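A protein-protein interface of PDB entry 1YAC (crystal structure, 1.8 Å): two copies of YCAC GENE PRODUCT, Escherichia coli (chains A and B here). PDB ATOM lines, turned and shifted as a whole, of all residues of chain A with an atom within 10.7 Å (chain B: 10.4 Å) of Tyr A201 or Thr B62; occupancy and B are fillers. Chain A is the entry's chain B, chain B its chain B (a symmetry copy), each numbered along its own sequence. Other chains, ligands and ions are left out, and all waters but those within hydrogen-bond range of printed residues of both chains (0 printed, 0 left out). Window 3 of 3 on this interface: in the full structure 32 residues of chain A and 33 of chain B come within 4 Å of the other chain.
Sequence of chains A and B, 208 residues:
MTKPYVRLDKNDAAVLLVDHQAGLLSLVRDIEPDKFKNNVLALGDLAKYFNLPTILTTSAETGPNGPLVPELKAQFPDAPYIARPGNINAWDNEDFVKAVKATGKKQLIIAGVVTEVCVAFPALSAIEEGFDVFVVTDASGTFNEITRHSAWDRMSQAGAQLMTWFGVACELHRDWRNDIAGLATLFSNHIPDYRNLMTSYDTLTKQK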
ATOM      1  N   TRP A 176       8.993  27.324   2.287  1.00  0.00           N
ATOM      2  CA  TRP A 176       8.715  25.952   1.862  1.00  0.00           C
ATOM      3  C   TRP A 176       7.255  25.575   2.127  1.00  0.00           C
ATOM      4  O   TRP A 176       6.568  25.033   1.257  1.00  0.00           O
ATOM      5  CB  TRP A 176       9.604  24.977   2.633  1.00  0.00           C
ATOM      6  CG  TRP A 176      10.943  24.741   2.037  1.00  0.00           C
ATOM      7  CD1 TRP A 176      12.137  25.274   2.449  1.00  0.00           C
ATOM      8  CD2 TRP A 176      11.255  23.850   0.955  1.00  0.00           C
ATOM      9  NE1 TRP A 176      13.168  24.762   1.696  1.00  0.00           N
ATOM     10  CE2 TRP A 176      12.656  23.885   0.772  1.00  0.00           C
ATOM     11  CE3 TRP A 176      10.477  23.023   0.122  1.00  0.00           C
ATOM     12  CZ2 TRP A 176      13.310  23.119  -0.208  1.00  0.00           C
ATOM     13  CZ3 TRP A 176      11.129  22.257  -0.858  1.00  0.00           C
ATOM     14  CH2 TRP A 176      12.531  22.314  -1.011  1.00  0.00           C
ATOM     15  N   ARG A 177       6.789  25.902   3.331  1.00  0.00           N
ATOM     16  CA  ARG A 177       5.434  25.591   3.772  1.00  0.00           C
ATOM     17  C   ARG A 177       4.310  26.081   2.861  1.00  0.00           C
ATOM     18  O   ARG A 177       3.190  25.585   2.949  1.00  0.00           O
ATOM     19  CB  ARG A 177       5.236  26.093   5.200  1.00  0.00           C
ATOM     20  CG  ARG A 177       6.174  25.419   6.195  1.00  0.00           C
ATOM     21  CD  ARG A 177       6.129  26.092   7.552  1.00  0.00           C
ATOM     22  NE  ARG A 177       6.703  27.435   7.518  1.00  0.00           N
ATOM     23  CZ  ARG A 177       6.740  28.256   8.561  1.00  0.00           C
ATOM     24  NH1 ARG A 177       6.234  27.873   9.725  1.00  0.00           N
ATOM     25  NH2 ARG A 177       7.292  29.457   8.446  1.00  0.00           N
ATOM     26  N   ILE A 180       5.308  22.626  -0.099  1.00  0.00           N
ATOM     27  CA  ILE A 180       6.522  21.818  -0.043  1.00  0.00           C
ATOM     28  C   ILE A 180       6.681  20.916  -1.255  1.00  0.00           C
ATOM     29  O   ILE A 180       7.682  20.995  -1.964  1.00  0.00           O
ATOM     30  CB  ILE A 180       6.577  20.965   1.263  1.00  0.00           C
ATOM     31  CG1 ILE A 180       6.763  21.875   2.481  1.00  0.00           C
ATOM     32  CG2 ILE A 180       7.713  19.923   1.191  1.00  0.00           C
ATOM     33  CD1 ILE A 180       6.807  21.131   3.810  1.00  0.00           C
ATOM     34  N   ALA A 184       9.623  21.086  -4.102  1.00  0.00           N
ATOM     35  CA  ALA A 184      10.460  19.891  -4.034  1.00  0.00           C
ATOM     36  C   ALA A 184      10.516  19.181  -5.386  1.00  0.00           C
ATOM     37  O   ALA A 184      11.571  18.693  -5.801  1.00  0.00           O
ATOM     38  CB  ALA A 184       9.947  18.947  -2.959  1.00  0.00           C
ATOM     39  N   ASP A 193      21.497  16.155  -7.809  1.00  0.00           N
ATOM     40  CA  ASP A 193      21.993  15.957  -6.442  1.00  0.00           C
ATOM     41  C   ASP A 193      20.845  16.020  -5.433  1.00  0.00           C
ATOM     42  O   ASP A 193      20.788  15.234  -4.484  1.00  0.00           O
ATOM     43  CB  ASP A 193      23.067  16.995  -6.076  1.00  0.00           C
ATOM     44  CG  ASP A 193      24.353  16.830  -6.878  1.00  0.00           C
ATOM     45  OD1 ASP A 193      24.808  15.685  -7.087  1.00  0.00           O
ATOM     46  OD2 ASP A 193      24.920  17.864  -7.292  1.00  0.00           O
ATOM     47  N   TYR A 194      19.915  16.938  -5.648  1.00  0.00           N
ATOM     48  CA  TYR A 194      18.800  17.044  -4.732  1.00  0.00           C
ATOM     49  C   TYR A 194      17.897  15.813  -4.882  1.00  0.00           C
ATOM     50  O   TYR A 194      17.431  15.239  -3.892  1.00  0.00           O
ATOM     51  CB  TYR A 194      18.017  18.327  -4.960  1.00  0.00           C
ATOM     52  CG  TYR A 194      17.198  18.674  -3.753  1.00  0.00           C
ATOM     53  CD1 TYR A 194      17.816  19.119  -2.581  1.00  0.00           C
ATOM     54  CD2 TYR A 194      15.816  18.527  -3.757  1.00  0.00           C
ATOM     55  CE1 TYR A 194      17.087  19.409  -1.442  1.00  0.00           C
ATOM     56  CE2 TYR A 194      15.062  18.818  -2.608  1.00  0.00           C
ATOM     57  CZ  TYR A 194      15.709  19.259  -1.460  1.00  0.00           C
ATOM     58  OH  TYR A 194      14.978  19.566  -0.330  1.00  0.00           O
ATOM     59  N   ARG A 195      17.664  15.400  -6.123  1.00  0.00           N
ATOM     60  CA  ARG A 195      16.849  14.221  -6.371  1.00  0.00           C
ATOM     61  C   ARG A 195      17.424  13.012  -5.626  1.00  0.00           C
ATOM     62  O   ARG A 195      16.673  12.230  -5.037  1.00  0.00           O
ATOM     63  CB  ARG A 195      16.746  13.925  -7.873  1.00  0.00           C
ATOM     64  CG  ARG A 195      16.034  12.609  -8.155  1.00  0.00           C
ATOM     65  CD  ARG A 195      15.660  12.443  -9.615  1.00  0.00           C
ATOM     66  NE  ARG A 195      14.470  13.207  -9.971  1.00  0.00           N
ATOM     67  CZ  ARG A 195      13.854  13.124 -11.145  1.00  0.00           C
ATOM     68  NH1 ARG A 195      14.311  12.307 -12.087  1.00  0.00           N
ATOM     69  NH2 ARG A 195      12.795  13.880 -11.383  1.00  0.00           N
ATOM     70  N   ASN A 196      18.750  12.880  -5.622  1.00  0.00           N
ATOM     71  CA  ASN A 196      19.416  11.757  -4.934  1.00  0.00           C
ATOM     72  C   ASN A 196      19.199  11.801  -3.422  1.00  0.00           C
ATOM     73  O   ASN A 196      18.975  10.769  -2.764  1.00  0.00           O
ATOM     74  CB  ASN A 196      20.912  11.729  -5.268  1.00  0.00           C
ATOM     75  CG  ASN A 196      21.177  11.342  -6.729  1.00  0.00           C
ATOM     76  OD1 ASN A 196      20.377  10.648  -7.351  1.00  0.00           O
ATOM     77  ND2 ASN A 196      22.287  11.805  -7.273  1.00  0.00           N
ATOM     78  N   LEU A 197      19.219  13.010  -2.880  1.00  0.00           N
ATOM     79  CA  LEU A 197      19.001  13.221  -1.462  1.00  0.00           C
ATOM     80  C   LEU A 197      17.576  12.772  -1.132  1.00  0.00           C
ATOM     81  O   LEU A 197      17.328  12.092  -0.135  1.00  0.00           O
ATOM     82  CB  LEU A 197      19.156  14.718  -1.176  1.00  0.00           C
ATOM     83  CG  LEU A 197      20.354  15.271  -0.407  1.00  0.00           C
ATOM     84  CD1 LEU A 197      21.566  14.469  -0.540  1.00  0.00           C
ATOM     85  CD2 LEU A 197      20.625  16.661  -0.820  1.00  0.00           C
ATOM     86  N   MET A 198      16.654  13.125  -2.012  1.00  0.00           N
ATOM     87  CA  MET A 198      15.251  12.790  -1.849  1.00  0.00           C
ATOM     88  C   MET A 198      15.037  11.271  -1.900  1.00  0.00           C
ATOM     89  O   MET A 198      14.346  10.691  -1.060  1.00  0.00           O
ATOM     90  CB  MET A 198      14.451  13.493  -2.944  1.00  0.00           C
ATOM     91  CG  MET A 198      13.044  13.827  -2.556  1.00  0.00           C
ATOM     92  SD  MET A 198      12.185  14.808  -3.790  1.00  0.00           S
ATOM     93  CE  MET A 198      13.151  16.150  -3.694  1.00  0.00           C
ATOM     94  N   THR A 199      15.678  10.623  -2.863  1.00  0.00           N
ATOM     95  CA  THR A 199      15.557   9.185  -3.019  1.00  0.00           C
ATOM     96  C   THR A 199      16.012   8.466  -1.755  1.00  0.00           C
ATOM     97  O   THR A 199      15.287   7.608  -1.223  1.00  0.00           O
ATOM     98  CB  THR A 199      16.374   8.704  -4.224  1.00  0.00           C
ATOM     99  OG1 THR A 199      15.860   9.316  -5.410  1.00  0.00           O
ATOM    100  CG2 THR A 199      16.305   7.188  -4.359  1.00  0.00           C
ATOM    101  N   SER A 200      17.191   8.819  -1.254  1.00  0.00           N
ATOM    102  CA  SER A 200      17.698   8.174  -0.047  1.00  0.00           C
ATOM    103  C   SER A 200      16.782   8.425   1.156  1.00  0.00           C
ATOM    104  O   SER A 200      16.444   7.492   1.896  1.00  0.00           O
ATOM    105  CB  SER A 200      19.120   8.644   0.261  1.00  0.00           C
ATOM    106  OG  SER A 200      20.004   8.275  -0.779  1.00  0.00           O
ATOM    107  N   TYR A 201      16.371   9.679   1.334  1.00  0.00           N
ATOM    108  CA  TYR A 201      15.495  10.050   2.442  1.00  0.00           C
ATOM    109  C   TYR A 201      14.157   9.309   2.376  1.00  0.00           C
ATOM    110  O   TYR A 201      13.709   8.741   3.371  1.00  0.00           O
ATOM    111  CB  TYR A 201      15.252  11.562   2.450  1.00  0.00           C
ATOM    112  CG  TYR A 201      14.348  12.015   3.573  1.00  0.00           C
ATOM    113  CD1 TYR A 201      14.840  12.172   4.867  1.00  0.00           C
ATOM    114  CD2 TYR A 201      12.990  12.224   3.354  1.00  0.00           C
ATOM    115  CE1 TYR A 201      14.002  12.516   5.910  1.00  0.00           C
ATOM    116  CE2 TYR A 201      12.145  12.566   4.387  1.00  0.00           C
ATOM    117  CZ  TYR A 201      12.656  12.706   5.661  1.00  0.00           C
ATOM    118  OH  TYR A 201      11.801  13.014   6.696  1.00  0.00           O
ATOM    119  N   ASP A 202      13.541   9.299   1.200  1.00  0.00           N
ATOM    120  CA  ASP A 202      12.264   8.633   1.011  1.00  0.00           C
ATOM    121  C   ASP A 202      12.313   7.131   1.256  1.00  0.00           C
ATOM    122  O   ASP A 202      11.437   6.583   1.917  1.00  0.00           O
ATOM    123  CB  ASP A 202      11.723   8.893  -0.395  1.00  0.00           C
ATOM    124  CG  ASP A 202      11.235  10.317  -0.585  1.00  0.00           C
ATOM    125  OD1 ASP A 202      11.177  11.074   0.409  1.00  0.00           O
ATOM    126  OD2 ASP A 202      10.901  10.677  -1.736  1.00  0.00           O
ATOM    127  N   THR A 203      13.314   6.446   0.712  1.00  0.00           N
ATOM    128  CA  THR A 203      13.365   5.006   0.903  1.00  0.00           C
ATOM    129  C   THR A 203      13.584   4.644   2.360  1.00  0.00           C
ATOM    130  O   THR A 203      13.132   3.596   2.810  1.00  0.00           O
ATOM    131  CB  THR A 203      14.423   4.325   0.024  1.00  0.00           C
ATOM    132  OG1 THR A 203      15.722   4.603   0.539  1.00  0.00           O
ATOM    133  CG2 THR A 203      14.349   4.846  -1.389  1.00  0.00           C
ATOM    134  N   LEU A 204      14.255   5.523   3.095  1.00  0.00           N
ATOM    135  CA  LEU A 204      14.536   5.301   4.508  1.00  0.00           C
ATOM    136  C   LEU A 204      13.379   5.614   5.444  1.00  0.00           C
ATOM    137  O   LEU A 204      13.264   5.004   6.504  1.00  0.00           O
ATOM    138  CB  LEU A 204      15.726   6.143   4.945  1.00  0.00           C
ATOM    139  CG  LEU A 204      17.144   5.626   4.786  1.00  0.00           C
ATOM    140  CD1 LEU A 204      18.077   6.598   5.460  1.00  0.00           C
ATOM    141  CD2 LEU A 204      17.266   4.262   5.452  1.00  0.00           C
ATOM    142  N   THR A 205      12.569   6.604   5.089  1.00  0.00           N
ATOM    143  CA  THR A 205      11.451   7.025   5.923  1.00  0.00           C
ATOM    144  C   THR A 205      10.093   6.481   5.484  1.00  0.00           C
ATOM    145  O   THR A 205       9.088   6.789   6.163  1.00  0.00           O
ATOM    146  CB  THR A 205      11.383   8.561   5.987  1.00  0.00           C
ATOM    147  OG1 THR A 205      11.113   9.091   4.681  1.00  0.00           O
ATOM    148  CG2 THR A 205      12.704   9.122   6.495  1.00  0.00           C
ATOM    149  N   GLN B  21      24.556  21.976   6.049  1.00  0.00           N
ATOM    150  CA  GLN B  21      23.956  20.691   6.366  1.00  0.00           C
ATOM    151  C   GLN B  21      24.501  19.535   5.529  1.00  0.00           C
ATOM    152  O   GLN B  21      24.880  19.713   4.369  1.00  0.00           O
ATOM    153  CB  GLN B  21      22.435  20.814   6.226  1.00  0.00           C
ATOM    154  CG  GLN B  21      21.826  21.787   7.245  1.00  0.00           C
ATOM    155  CD  GLN B  21      20.435  22.292   6.856  1.00  0.00           C
ATOM    156  OE1 GLN B  21      20.267  23.518   6.689  1.00  0.00           O
ATOM    157  NE2 GLN B  21      19.507  21.465   6.716  1.00  0.00           N
ATOM    158  N   ALA B  22      24.515  18.348   6.126  1.00  0.00           N
ATOM    159  CA  ALA B  22      25.039  17.156   5.464  1.00  0.00           C
ATOM    160  C   ALA B  22      24.486  16.904   4.047  1.00  0.00           C
ATOM    161  O   ALA B  22      25.251  16.590   3.127  1.00  0.00           O
ATOM    162  CB  ALA B  22      24.828  15.943   6.346  1.00  0.00           C
ATOM    163  N   GLY B  23      23.175  17.050   3.873  1.00  0.00           N
ATOM    164  CA  GLY B  23      22.575  16.828   2.568  1.00  0.00           C
ATOM    165  C   GLY B  23      22.928  17.955   1.610  1.00  0.00           C
ATOM    166  O   GLY B  23      23.468  17.725   0.523  1.00  0.00           O
ATOM    167  N   LEU B  24      22.693  19.190   2.047  1.00  0.00           N
ATOM    168  CA  LEU B  24      22.981  20.364   1.227  1.00  0.00           C
ATOM    169  C   LEU B  24      24.437  20.467   0.757  1.00  0.00           C
ATOM    170  O   LEU B  24      24.701  21.025  -0.304  1.00  0.00           O
ATOM    171  CB  LEU B  24      22.570  21.641   1.964  1.00  0.00           C
ATOM    172  CG  LEU B  24      21.065  21.813   2.209  1.00  0.00           C
ATOM    173  CD1 LEU B  24      20.837  23.091   2.978  1.00  0.00           C
ATOM    174  CD2 LEU B  24      20.304  21.847   0.899  1.00  0.00           C
ATOM    175  N   THR B  58      19.454  26.205  10.321  1.00  0.00           N
ATOM    176  CA  THR B  58      19.284  25.149   9.325  1.00  0.00           C
ATOM    177  C   THR B  58      17.934  25.297   8.644  1.00  0.00           C
ATOM    178  O   THR B  58      17.014  25.901   9.199  1.00  0.00           O
ATOM    179  CB  THR B  58      19.354  23.729   9.946  1.00  0.00           C
ATOM    180  OG1 THR B  58      18.303  23.565  10.906  1.00  0.00           O
ATOM    181  CG2 THR B  58      20.712  23.481  10.606  1.00  0.00           C
ATOM    182  N   SER B  59      17.797  24.671   7.476  1.00  0.00           N
ATOM    183  CA  SER B  59      16.562  24.724   6.701  1.00  0.00           C
ATOM    184  C   SER B  59      16.055  23.307   6.498  1.00  0.00           C
ATOM    185  O   SER B  59      16.782  22.451   5.977  1.00  0.00           O
ATOM    186  CB  SER B  59      16.835  25.386   5.345  1.00  0.00           C
ATOM    187  OG  SER B  59      15.773  25.177   4.433  1.00  0.00           O
ATOM    188  N   ALA B  60      14.844  23.058   6.990  1.00  0.00           N
ATOM    189  CA  ALA B  60      14.191  21.751   6.870  1.00  0.00           C
ATOM    190  C   ALA B  60      15.150  20.581   7.097  1.00  0.00           C
ATOM    191  O   ALA B  60      15.197  19.644   6.304  1.00  0.00           O
ATOM    192  CB  ALA B  60      13.492  21.639   5.506  1.00  0.00           C
ATOM    193  N   GLU B  61      15.885  20.632   8.205  1.00  0.00           N
ATOM    194  CA  GLU B  61      16.865  19.602   8.528  1.00  0.00           C
ATOM    195  C   GLU B  61      16.331  18.184   8.644  1.00  0.00           C
ATOM    196  O   GLU B  61      17.109  17.235   8.590  1.00  0.00           O
ATOM    197  CB  GLU B  61      17.653  19.974   9.788  1.00  0.00           C
ATOM    198  CG  GLU B  61      16.820  20.009  11.057  1.00  0.00           C
ATOM    199  CD  GLU B  61      17.619  20.429  12.286  1.00  0.00           C
ATOM    200  OE1 GLU B  61      18.548  21.261  12.160  1.00  0.00           O
ATOM    201  OE2 GLU B  61      17.303  19.936  13.390  1.00  0.00           O
ATOM    202  N   THR B  62      15.026  18.039   8.857  1.00  0.00           N
ATOM    203  CA  THR B  62      14.420  16.710   8.959  1.00  0.00           C
ATOM    204  C   THR B  62      13.806  16.413   7.602  1.00  0.00           C
ATOM    205  O   THR B  62      12.596  16.432   7.416  1.00  0.00           O
ATOM    206  CB  THR B  62      13.340  16.655  10.052  1.00  0.00           C
ATOM    207  OG1 THR B  62      12.444  17.765   9.892  1.00  0.00           O
ATOM    208  CG2 THR B  62      13.988  16.703  11.432  1.00  0.00           C
ATOM    209  N   GLY B  63      14.675  16.199   6.640  1.00  0.00           N
ATOM    210  CA  GLY B  63      14.248  15.933   5.291  1.00  0.00           C
ATOM    211  C   GLY B  63      15.542  15.726   4.548  1.00  0.00           C
ATOM    212  O   GLY B  63      16.598  15.606   5.179  1.00  0.00           O
ATOM    213  N   PRO B  64      15.511  15.725   3.213  1.00  0.00           N
ATOM    214  CA  PRO B  64      16.709  15.531   2.391  1.00  0.00           C
ATOM    215  C   PRO B  64      17.869  16.477   2.741  1.00  0.00           C
ATOM    216  O   PRO B  64      19.025  16.103   2.585  1.00  0.00           O
ATOM    217  CB  PRO B  64      16.193  15.813   0.978  1.00  0.00           C
ATOM    218  CG  PRO B  64      14.752  15.457   1.056  1.00  0.00           C
ATOM    219  CD  PRO B  64      14.331  16.005   2.382  1.00  0.00           C
ATOM    220  N   ASN B  65      17.553  17.709   3.165  1.00  0.00           N
ATOM    221  CA  ASN B  65      18.582  18.712   3.506  1.00  0.00           C
ATOM    222  C   ASN B  65      19.562  18.181   4.543  1.00  0.00           C
ATOM    223  O   ASN B  65      20.770  18.475   4.501  1.00  0.00           O
ATOM    224  CB  ASN B  65      17.950  20.037   3.976  1.00  0.00           C
ATOM    225  CG  ASN B  65      17.314  20.822   2.829  1.00  0.00           C
ATOM    226  OD1 ASN B  65      17.255  20.340   1.693  1.00  0.00           O
ATOM    227  ND2 ASN B  65      16.816  22.019   3.118  1.00  0.00           N
ATOM    228  N   GLY B  66      19.046  17.381   5.465  1.00  0.00           N
ATOM    229  CA  GLY B  66      19.912  16.792   6.457  1.00  0.00           C
ATOM    230  C   GLY B  66      20.270  17.664   7.638  1.00  0.00           C
ATOM    231  O   GLY B  66      19.994  18.872   7.658  1.00  0.00           O
ATOM    232  N   PRO B  67      20.928  17.067   8.639  1.00  0.00           N
ATOM    233  CA  PRO B  67      21.340  17.757   9.861  1.00  0.00           C
ATOM    234  C   PRO B  67      22.543  18.647   9.675  1.00  0.00           C
ATOM    235  O   PRO B  67      23.254  18.545   8.670  1.00  0.00           O
ATOM    236  CB  PRO B  67      21.662  16.599  10.802  1.00  0.00           C
ATOM    237  CG  PRO B  67      22.214  15.563   9.878  1.00  0.00           C
ATOM    238  CD  PRO B  67      21.306  15.638   8.675  1.00  0.00           C
ATOM    239  N   LEU B  68      22.752  19.550  10.628  1.00  0.00           N
ATOM    240  CA  LEU B  68      23.914  20.423  10.575  1.00  0.00           C
ATOM    241  C   LEU B  68      25.151  19.520  10.688  1.00  0.00           C
ATOM    242  O   LEU B  68      25.103  18.494  11.384  1.00  0.00           O
ATOM    243  CB  LEU B  68      23.887  21.402  11.758  1.00  0.00           C
ATOM    244  CG  LEU B  68      24.958  22.498  11.756  1.00  0.00           C
ATOM    245  CD1 LEU B  68      24.692  23.489  10.611  1.00  0.00           C
ATOM    246  CD2 LEU B  68      24.954  23.214  13.091  1.00  0.00           C
ATOM    247  N   TYR B  81      20.487  28.185  17.992  1.00  0.00           N
ATOM    248  CA  TYR B  81      20.365  27.211  16.912  1.00  0.00           C
ATOM    249  C   TYR B  81      18.923  27.307  16.433  1.00  0.00           C
ATOM    250  O   TYR B  81      17.999  26.856  17.124  1.00  0.00           O
ATOM    251  CB  TYR B  81      20.660  25.821  17.467  1.00  0.00           C
ATOM    252  CG  TYR B  81      20.707  24.722  16.438  1.00  0.00           C
ATOM    253  CD1 TYR B  81      19.578  24.387  15.684  1.00  0.00           C
ATOM    254  CD2 TYR B  81      21.877  24.005  16.224  1.00  0.00           C
ATOM    255  CE1 TYR B  81      19.619  23.359  14.741  1.00  0.00           C
ATOM    256  CE2 TYR B  81      21.928  22.980  15.290  1.00  0.00           C
ATOM    257  CZ  TYR B  81      20.797  22.667  14.555  1.00  0.00           C
ATOM    258  OH  TYR B  81      20.854  21.652  13.641  1.00  0.00           O
ATOM    259  N   ILE B  82      18.723  27.942  15.285  1.00  0.00           N
ATOM    260  CA  ILE B  82      17.378  28.131  14.755  1.00  0.00           C
ATOM    261  C   ILE B  82      17.077  27.161  13.616  1.00  0.00           C
ATOM    262  O   ILE B  82      17.646  27.275  12.531  1.00  0.00           O
ATOM    263  CB  ILE B  82      17.155  29.604  14.262  1.00  0.00           C
ATOM    264  CG1 ILE B  82      17.362  30.619  15.394  1.00  0.00           C
ATOM    265  CG2 ILE B  82      15.748  29.769  13.701  1.00  0.00           C
ATOM    266  CD1 ILE B  82      18.787  31.076  15.586  1.00  0.00           C
ATOM    267  N   ALA B  83      16.250  26.161  13.886  1.00  0.00           N
ATOM    268  CA  ALA B  83      15.858  25.210  12.850  1.00  0.00           C
ATOM    269  C   ALA B  83      14.656  25.844  12.170  1.00  0.00           C
ATOM    270  O   ALA B  83      13.571  25.912  12.752  1.00  0.00           O
ATOM    271  CB  ALA B  83      15.476  23.870  13.464  1.00  0.00           C
ATOM    272  N   ARG B  84      14.855  26.368  10.965  1.00  0.00           N
ATOM    273  CA  ARG B  84      13.782  27.010  10.224  1.00  0.00           C
ATOM    274  C   ARG B  84      12.952  25.945   9.530  1.00  0.00           C
ATOM    275  O   ARG B  84      13.477  25.128   8.764  1.00  0.00           O
ATOM    276  CB  ARG B  84      14.357  27.979   9.186  1.00  0.00           C
ATOM    277  CG  ARG B  84      15.465  28.862   9.736  1.00  0.00           C
ATOM    278  CD  ARG B  84      15.775  30.050   8.831  1.00  0.00           C
ATOM    279  NE  ARG B  84      16.050  29.709   7.433  1.00  0.00           N
ATOM    280  CZ  ARG B  84      17.145  29.098   6.984  1.00  0.00           C
ATOM    281  NH1 ARG B  84      18.116  28.734   7.809  1.00  0.00           N
ATOM    282  NH2 ARG B  84      17.263  28.825   5.695  1.00  0.00           N
ATOM    283  N   PRO B  85      11.636  25.933   9.791  1.00  0.00           N
ATOM    284  CA  PRO B  85      10.738  24.949   9.181  1.00  0.00           C
ATOM    285  C   PRO B  85      10.252  25.287   7.779  1.00  0.00           C
ATOM    286  O   PRO B  85       9.588  24.463   7.155  1.00  0.00           O
ATOM    287  CB  PRO B  85       9.549  24.901  10.143  1.00  0.00           C
ATOM    288  CG  PRO B  85       9.764  26.018  11.137  1.00  0.00           C
ATOM    289  CD  PRO B  85      10.891  26.865  10.648  1.00  0.00           C
ATOM    290  N   GLY B  86      10.574  26.475   7.276  1.00  0.00           N
ATOM    291  CA  GLY B  86      10.088  26.839   5.957  1.00  0.00           C
ATOM    292  C   GLY B  86      10.683  28.076   5.318  1.00  0.00           C
ATOM    293  O   GLY B  86      10.799  28.131   4.096  1.00  0.00           O
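The backbone NH (N) of Trp A176 sits at hydrogen-bond distance from the backbone carbonyl oxygen (O) of Gly B86, 2.7 Å away. OH of Tyr A194 is in hydrogen-bond range of OD1 of Asn B65 (3.1 Å).
N of Ser B59 lies within hydrogen-bond range of OE1 of Gln B21, 2.8 Å away. The backbone NH (N) of Leu B24 sits at hydrogen-bond distance from the backbone carbonyl oxygen (O) of Asn B65, 3.2 Å away. N of Gly B23 is in hydrogen-bond range of O of Asn B65, at 2.9 Å. The backbone carbonyl oxygen of Ser B59 sits at hydrogen-bond distance from the side-chain amide nitrogen of Asn B65, at 2.9 Å. The backbone carbonyl oxygen (O) of Tyr A201 sits at hydrogen-bond distance from the side-chain hydroxyl (OG1) of Thr A205 (2.9 Å).
Ser B59 touches Trp A176 (OG to NE1, 3.8 Å). O of Pro B85 touches CG of Arg A177 (3.7 Å). NE of Arg A177 touches CA of Gly B86 (3.8 Å). Gly B23 touches Leu A197 (O to CD2, 3.3 Å). CG of Leu A197 touches O of Pro B64, at 3.4 Å. Pro B64 touches Met A198. Thr B62 touches Tyr A201. Tyr A201 touches Gly B63 (CE1 to CA, 3.5 Å). N of Pro B64 touches CG of Tyr A201, 3.9 Å away.
Printed residues of chain B within 4 Å of Trp A176: Ser B59 and Gly B86. Ile A180 touches none of the printed residues of chain B. Printed residues of chain B within 4 Å of Leu A197: Gly B23 (3.3 Å) and Pro B64 (3.4 Å). No residue of chain B comes within 4 Å of Ser A200. Of chain B, only Thr B62 (3.6 Å), Gly B63 (3.5 Å) and Pro B64 (3.9 Å) come within 4 Å of Tyr A201. No residue of chain B comes within 4 Å of Leu A204. No residue of chain B comes within 4 Å of Thr A205. Printed residues of chain A within 4 Å of Gly B23: Leu A197. No residue of chain A comes within 4 Å of Ala B60. Thr B62 touches one residue of chain A. Of chain A, only Leu A197 (3.4 Å), Met A198 (3.98 Å) and Tyr A201 (3.9 Å) come within 4 Å of Pro B64. Of the printed residues of chain A, Asn B65 touches Tyr A194 (3.1 Å). Arg B84 touches none of the printed residues of chain A. Of the printed residues of chain A, Gly B86 touches Trp A176 (2.7 Å) and Arg A177 (3.8 Å). The nearest residue of chain B that does not touch Tyr A201 is Glu B61 (6.3 Å). The nearest residue of chain A that does not touch Thr B62 is Thr A205 (7.4 Å). The nearest printed residue of chain B that does not touch Met A198 is Asn B65 (7.0 Å).
Of the 17 printed residues of chain A, 6 touch a printed residue of chain B. Hydrophobic or aromatic side chains of chain A that line the printed part of chain B: Trp A176, Tyr A194, Leu A197 and Tyr A201. Printed residues of chain B that touch a printed residue of chain A: Gly B23, Ser B59, Thr B62, Gly B63, Pro B64, Asn B65, Pro B85 and Gly B86. Hydrophobic or aromatic side chains of chain B within 4 Å of the printed part of chain A: Pro B64. Among the printed residues, no Asp or Glu carboxylate lies within 4 Å of a Lys or Arg side-chain nitrogen of the other chain.
No position is printed for both chains. Of the 11 pairs that touch across the chains among the printed residues, none has its exchanged pair printed and touching as well.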
